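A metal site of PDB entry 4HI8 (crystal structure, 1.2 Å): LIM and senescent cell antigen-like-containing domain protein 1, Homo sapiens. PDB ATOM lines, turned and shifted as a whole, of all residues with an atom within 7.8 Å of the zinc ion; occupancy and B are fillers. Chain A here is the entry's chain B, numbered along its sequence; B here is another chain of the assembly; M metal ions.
The nearest printed residue that does not touch the zinc ion is Gln 44 (4.5 Å).
The side-chain carboxylate of Asp 66 sits at hydrogen-bond distance from a ring nitrogen (NE2) of His 104 of chain B (2.8 Å).
N of Gln 47 lies close to SG of Cys 45 (3.6 Å).
The side-chain sulfur (SG) of Cys 42 sits close to the backbone NH (N) of Gln 44 (3.3 Å).
The backbone NH (N) of Cys 42 is in hydrogen-bond range of the backbone carbonyl oxygen (O) of Gln 47 (2.9 Å).
The backbone NH of His 65 lies close to the side-chain sulfur of Cys 63 (3.8 Å).
The zinc ion is bound by OD2 of Asp 66, SG of Cys 45, SG of Cys 42 and SG of Cys 63.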
ATOM      1  N   VAL A  41     -12.572  24.831   2.741  1.00  0.00           N
ATOM      2  CA  VAL A  41     -12.155  24.263   4.000  1.00  0.00           C
ATOM      3  C   VAL A  41     -13.115  24.783   5.076  1.00  0.00           C
ATOM      4  O   VAL A  41     -13.776  25.782   4.912  1.00  0.00           O
ATOM      5  CB  VAL A  41     -10.692  24.663   4.374  1.00  0.00           C
ATOM      6  CG1 VAL A  41      -9.672  24.192   3.306  1.00  0.00           C
ATOM      7  CG2 VAL A  41     -10.562  26.184   4.652  1.00  0.00           C
ATOM      8  N   CYS A  42     -13.109  24.097   6.208  1.00  0.00           N
ATOM      9  CA  CYS A  42     -13.917  24.514   7.347  1.00  0.00           C
ATOM     10  C   CYS A  42     -13.484  25.858   7.889  1.00  0.00           C
ATOM     11  O   CYS A  42     -12.274  26.094   8.105  1.00  0.00           O
ATOM     12  CB  CYS A  42     -13.712  23.472   8.454  1.00  0.00           C
ATOM     13  SG  CYS A  42     -14.626  23.878  10.004  1.00  0.00           S
ATOM     14  N   ALA A  43     -14.455  26.731   8.151  1.00  0.00           N
ATOM     15  CA  ALA A  43     -14.145  28.070   8.664  1.00  0.00           C
ATOM     16  C   ALA A  43     -13.540  28.059  10.068  1.00  0.00           C
ATOM     17  O   ALA A  43     -12.906  29.030  10.485  1.00  0.00           O
ATOM     18  CB  ALA A  43     -15.422  28.920   8.659  1.00  0.00           C
ATOM     19  N   GLN A  44     -13.795  26.989  10.852  1.00  0.00           N
ATOM     20  CA  GLN A  44     -13.264  26.925  12.209  1.00  0.00           C
ATOM     21  C   GLN A  44     -11.880  26.295  12.325  1.00  0.00           C
ATOM     22  O   GLN A  44     -11.030  26.799  13.032  1.00  0.00           O
ATOM     23  CB  GLN A  44     -14.256  26.153  13.084  1.00  0.00           C
ATOM     24  CG  GLN A  44     -13.987  26.310  14.589  1.00  0.00           C
ATOM     25  CD  GLN A  44     -14.302  27.751  15.071  1.00  0.00           C
ATOM     26  OE1 GLN A  44     -14.849  28.573  14.327  1.00  0.00           O
ATOM     27  NE2 GLN A  44     -13.904  28.035  16.309  1.00  0.00           N
ATOM     28  N   CYS A  45     -11.639  25.176  11.629  1.00  0.00           N
ATOM     29  CA  CYS A  45     -10.373  24.437  11.755  1.00  0.00           C
ATOM     30  C   CYS A  45      -9.442  24.636  10.545  1.00  0.00           C
ATOM     31  O   CYS A  45      -8.277  24.287  10.660  1.00  0.00           O
ATOM     32  CB  CYS A  45     -10.591  22.949  12.021  1.00  0.00           C
ATOM     33  SG  CYS A  45     -11.434  22.066  10.646  1.00  0.00           S
ATOM     34  N   PHE A  46      -9.969  25.182   9.442  1.00  0.00           N
ATOM     35  CA  PHE A  46      -9.263  25.480   8.189  1.00  0.00           C
ATOM     36  C   PHE A  46      -8.835  24.214   7.432  1.00  0.00           C
ATOM     37  O   PHE A  46      -8.034  24.300   6.488  1.00  0.00           O
ATOM     38  CB  PHE A  46      -8.020  26.383   8.359  1.00  0.00           C
ATOM     39  CG  PHE A  46      -8.217  27.547   9.335  1.00  0.00           C
ATOM     40  CD1 PHE A  46      -9.341  28.382   9.261  1.00  0.00           C
ATOM     41  CD2 PHE A  46      -7.271  27.801  10.318  1.00  0.00           C
ATOM     42  CE1 PHE A  46      -9.493  29.452  10.112  1.00  0.00           C
ATOM     43  CE2 PHE A  46      -7.410  28.874  11.185  1.00  0.00           C
ATOM     44  CZ  PHE A  46      -8.560  29.694  11.068  1.00  0.00           C
ATOM     45  N   GLN A  47      -9.383  23.043   7.796  1.00  0.00           N
ATOM     46  CA  GLN A  47      -9.014  21.811   7.146  1.00  0.00           C
ATOM     47  C   GLN A  47     -10.072  21.402   6.136  1.00  0.00           C
ATOM     48  O   GLN A  47     -11.168  21.917   6.119  1.00  0.00           O
ATOM     49  CB  GLN A  47      -8.779  20.708   8.200  1.00  0.00           C
ATOM     50  CG  GLN A  47      -7.650  21.038   9.152  1.00  0.00           C
ATOM     51  CD  GLN A  47      -6.249  20.975   8.501  1.00  0.00           C
ATOM     52  OE1 GLN A  47      -5.943  20.060   7.796  1.00  0.00           O
ATOM     53  NE2 GLN A  47      -5.379  21.939   8.805  1.00  0.00           N
ATOM     54  N   GLN A  48      -9.686  20.498   5.250  1.00  0.00           N
ATOM     55  CA  GLN A  48     -10.619  19.925   4.271  1.00  0.00           C
ATOM     56  C   GLN A  48     -11.764  19.187   4.966  1.00  0.00           C
ATOM     57  O   GLN A  48     -11.622  18.580   6.065  1.00  0.00           O
ATOM     58  CB  GLN A  48      -9.853  18.994   3.303  1.00  0.00           C
ATOM     59  CG  GLN A  48      -8.891  19.795   2.459  1.00  0.00           C
ATOM     60  CD  GLN A  48      -8.115  19.010   1.447  1.00  0.00           C
ATOM     61  OE1 GLN A  48      -8.445  17.867   1.125  1.00  0.00           O
ATOM     62  NE2 GLN A  48      -7.072  19.628   0.918  1.00  0.00           N
ATOM     63  N   PHE A  49     -12.928  19.230   4.356  1.00  0.00           N
ATOM     64  CA  PHE A  49     -14.074  18.535   4.915  1.00  0.00           C
ATOM     65  C   PHE A  49     -13.954  17.009   4.733  1.00  0.00           C
ATOM     66  O   PHE A  49     -13.819  16.530   3.603  1.00  0.00           O
ATOM     67  CB  PHE A  49     -15.358  19.009   4.213  1.00  0.00           C
ATOM     68  CG  PHE A  49     -15.616  20.486   4.293  1.00  0.00           C
ATOM     69  CD1 PHE A  49     -15.901  21.117   5.506  1.00  0.00           C
ATOM     70  CD2 PHE A  49     -15.527  21.291   3.143  1.00  0.00           C
ATOM     71  CE1 PHE A  49     -16.139  22.465   5.565  1.00  0.00           C
ATOM     72  CE2 PHE A  49     -15.769  22.632   3.207  1.00  0.00           C
ATOM     73  CZ  PHE A  49     -16.048  23.243   4.418  1.00  0.00           C
ATOM     74  N   PRO A  50     -14.059  16.209   5.818  1.00  0.00           N
ATOM     75  CA  PRO A  50     -14.034  14.747   5.574  1.00  0.00           C
ATOM     76  C   PRO A  50     -15.179  14.333   4.648  1.00  0.00           C
ATOM     77  O   PRO A  50     -16.318  14.718   4.881  1.00  0.00           O
ATOM     78  CB  PRO A  50     -14.214  14.143   6.971  1.00  0.00           C
ATOM     79  CG  PRO A  50     -13.740  15.232   7.923  1.00  0.00           C
ATOM     80  CD  PRO A  50     -14.127  16.539   7.255  1.00  0.00           C
ATOM     81  N   LYS A  61     -19.037  27.791   6.177  1.00  0.00           N
ATOM     82  CA  LYS A  61     -19.145  26.335   6.026  1.00  0.00           C
ATOM     83  C   LYS A  61     -18.260  25.693   7.089  1.00  0.00           C
ATOM     84  O   LYS A  61     -17.121  26.124   7.253  1.00  0.00           O
ATOM     85  CB  LYS A  61     -18.614  25.920   4.644  1.00  0.00           C
ATOM     86  CG  LYS A  61     -19.447  26.480   3.500  1.00  0.00           C
ATOM     87  CD  LYS A  61     -18.923  26.087   2.121  1.00  0.00           C
ATOM     88  CE  LYS A  61     -19.892  26.520   0.965  1.00  0.00           C
ATOM     89  NZ  LYS A  61     -20.117  27.989   1.085  1.00  0.00           N
ATOM     90  N   TYR A  62     -18.794  24.690   7.776  1.00  0.00           N
ATOM     91  CA  TYR A  62     -18.120  24.034   8.869  1.00  0.00           C
ATOM     92  C   TYR A  62     -18.141  22.498   8.636  1.00  0.00           C
ATOM     93  O   TYR A  62     -19.097  21.933   8.114  1.00  0.00           O
ATOM     94  CB  TYR A  62     -18.787  24.322  10.240  1.00  0.00           C
ATOM     95  CG  TYR A  62     -18.757  25.810  10.552  1.00  0.00           C
ATOM     96  CD1 TYR A  62     -17.699  26.392  11.235  1.00  0.00           C
ATOM     97  CD2 TYR A  62     -19.778  26.653  10.122  1.00  0.00           C
ATOM     98  CE1 TYR A  62     -17.632  27.791  11.480  1.00  0.00           C
ATOM     99  CE2 TYR A  62     -19.724  28.025  10.395  1.00  0.00           C
ATOM    100  CZ  TYR A  62     -18.665  28.585  11.068  1.00  0.00           C
ATOM    101  OH  TYR A  62     -18.689  29.962  11.313  1.00  0.00           O
ATOM    102  N   CYS A  63     -17.084  21.834   9.111  1.00  0.00           N
ATOM    103  CA  CYS A  63     -17.075  20.371   9.164  1.00  0.00           C
ATOM    104  C   CYS A  63     -18.033  19.870  10.227  1.00  0.00           C
ATOM    105  O   CYS A  63     -18.508  20.623  11.093  1.00  0.00           O
ATOM    106  CB  CYS A  63     -15.696  19.798   9.430  1.00  0.00           C
ATOM    107  SG  CYS A  63     -15.043  20.209  11.166  1.00  0.00           S
ATOM    108  N   GLU A  64     -18.383  18.585  10.138  1.00  0.00           N
ATOM    109  CA  GLU A  64     -19.275  17.990  11.137  1.00  0.00           C
ATOM    110  C   GLU A  64     -18.823  18.253  12.555  1.00  0.00           C
ATOM    111  O   GLU A  64     -19.645  18.615  13.429  1.00  0.00           O
ATOM    112  CB  GLU A  64     -19.322  16.487  10.905  1.00  0.00           C
ATOM    113  CG  GLU A  64     -20.383  15.796  11.784  1.00  0.00           C
ATOM    114  CD  GLU A  64     -20.613  14.364  11.416  1.00  0.00           C
ATOM    115  OE1 GLU A  64     -19.926  13.808  10.554  1.00  0.00           O
ATOM    116  OE2 GLU A  64     -21.504  13.764  12.000  1.00  0.00           O
ATOM    117  N   HIS A  65     -17.558  17.989  12.861  1.00  0.00           N
ATOM    118  CA  HIS A  65     -17.059  18.193  14.225  1.00  0.00           C
ATOM    119  C   HIS A  65     -17.316  19.593  14.744  1.00  0.00           C
ATOM    120  O   HIS A  65     -17.883  19.761  15.833  1.00  0.00           O
ATOM    121  CB  HIS A  65     -15.574  17.882  14.310  1.00  0.00           C
ATOM    122  CG  HIS A  65     -14.950  18.172  15.637  1.00  0.00           C
ATOM    123  ND1 HIS A  65     -15.158  17.381  16.751  1.00  0.00           N
ATOM    124  CD2 HIS A  65     -14.283  19.261  16.072  1.00  0.00           C
ATOM    125  CE1 HIS A  65     -14.552  17.946  17.775  1.00  0.00           C
ATOM    126  NE2 HIS A  65     -13.995  19.074  17.398  1.00  0.00           N
ATOM    127  N   ASP A  66     -16.939  20.603  13.976  1.00  0.00           N
ATOM    128  CA  ASP A  66     -17.067  21.951  14.451  1.00  0.00           C
ATOM    129  C   ASP A  66     -18.509  22.453  14.455  1.00  0.00           C
ATOM    130  O   ASP A  66     -18.914  23.213  15.342  1.00  0.00           O
ATOM    131  CB  ASP A  66     -16.152  22.841  13.606  1.00  0.00           C
ATOM    132  CG  ASP A  66     -14.694  22.725  14.030  1.00  0.00           C
ATOM    133  OD1 ASP A  66     -14.442  22.758  15.232  1.00  0.00           O
ATOM    134  OD2 ASP A  66     -13.778  22.594  13.171  1.00  0.00           O
ATOM    135  N   PHE A  67     -19.323  22.013  13.501  1.00  0.00           N
ATOM    136  CA  PHE A  67     -20.745  22.324  13.495  1.00  0.00           C
ATOM    137  C   PHE A  67     -21.413  21.761  14.772  1.00  0.00           C
ATOM    138  O   PHE A  67     -22.203  22.438  15.427  1.00  0.00           O
ATOM    139  CB  PHE A  67     -21.423  21.854  12.202  1.00  0.00           C
ATOM    140  CG  PHE A  67     -22.858  22.302  12.080  1.00  0.00           C
ATOM    141  CD1 PHE A  67     -23.158  23.549  11.610  1.00  0.00           C
ATOM    142  CD2 PHE A  67     -23.913  21.499  12.480  1.00  0.00           C
ATOM    143  CE1 PHE A  67     -24.473  23.982  11.523  1.00  0.00           C
ATOM    144  CE2 PHE A  67     -25.216  21.925  12.397  1.00  0.00           C
ATOM    145  CZ  PHE A  67     -25.482  23.176  11.925  1.00  0.00           C
ATOM    146  N   HIS B 104      -8.472  24.002  18.439  1.00  0.00           N
ATOM    147  CA  HIS B 104      -7.598  23.703  17.292  1.00  0.00           C
ATOM    148  C   HIS B 104      -6.269  24.360  17.421  1.00  0.00           C
ATOM    149  O   HIS B 104      -5.423  24.237  16.488  1.00  0.00           O
ATOM    150  CB  HIS B 104      -8.302  24.107  15.980  1.00  0.00           C
ATOM    151  CG  HIS B 104      -9.581  23.394  15.743  1.00  0.00           C
ATOM    152  ND1 HIS B 104      -9.635  22.038  15.493  1.00  0.00           N
ATOM    153  CD2 HIS B 104     -10.861  23.848  15.780  1.00  0.00           C
ATOM    154  CE1 HIS B 104     -10.910  21.702  15.385  1.00  0.00           C
ATOM    155  NE2 HIS B 104     -11.675  22.777  15.577  1.00  0.00           N
ATOM    156  N   TYR B 137      -2.290  21.987  13.844  1.00  0.00           N
ATOM    157  CA  TYR B 137      -2.085  21.339  12.530  1.00  0.00           C
ATOM    158  C   TYR B 137      -0.866  22.026  11.836  1.00  0.00           C
ATOM    159  O   TYR B 137      -0.655  21.853  10.633  1.00  0.00           O
ATOM    160  CB  TYR B 137      -3.372  21.397  11.667  1.00  0.00           C
ATOM    161  CG  TYR B 137      -4.552  21.028  12.523  1.00  0.00           C
ATOM    162  CD1 TYR B 137      -4.560  19.844  13.309  1.00  0.00           C
ATOM    163  CD2 TYR B 137      -5.625  21.909  12.659  1.00  0.00           C
ATOM    164  CE1 TYR B 137      -5.625  19.587  14.196  1.00  0.00           C
ATOM    165  CE2 TYR B 137      -6.700  21.597  13.499  1.00  0.00           C
ATOM    166  CZ  TYR B 137      -6.649  20.483  14.303  1.00  0.00           C
ATOM    167  OH  TYR B 137      -7.651  20.184  15.211  1.00  0.00           O
HETATM  168 ZN    ZN M   1     -13.686  22.116  11.221  1.00  0.00          ZN
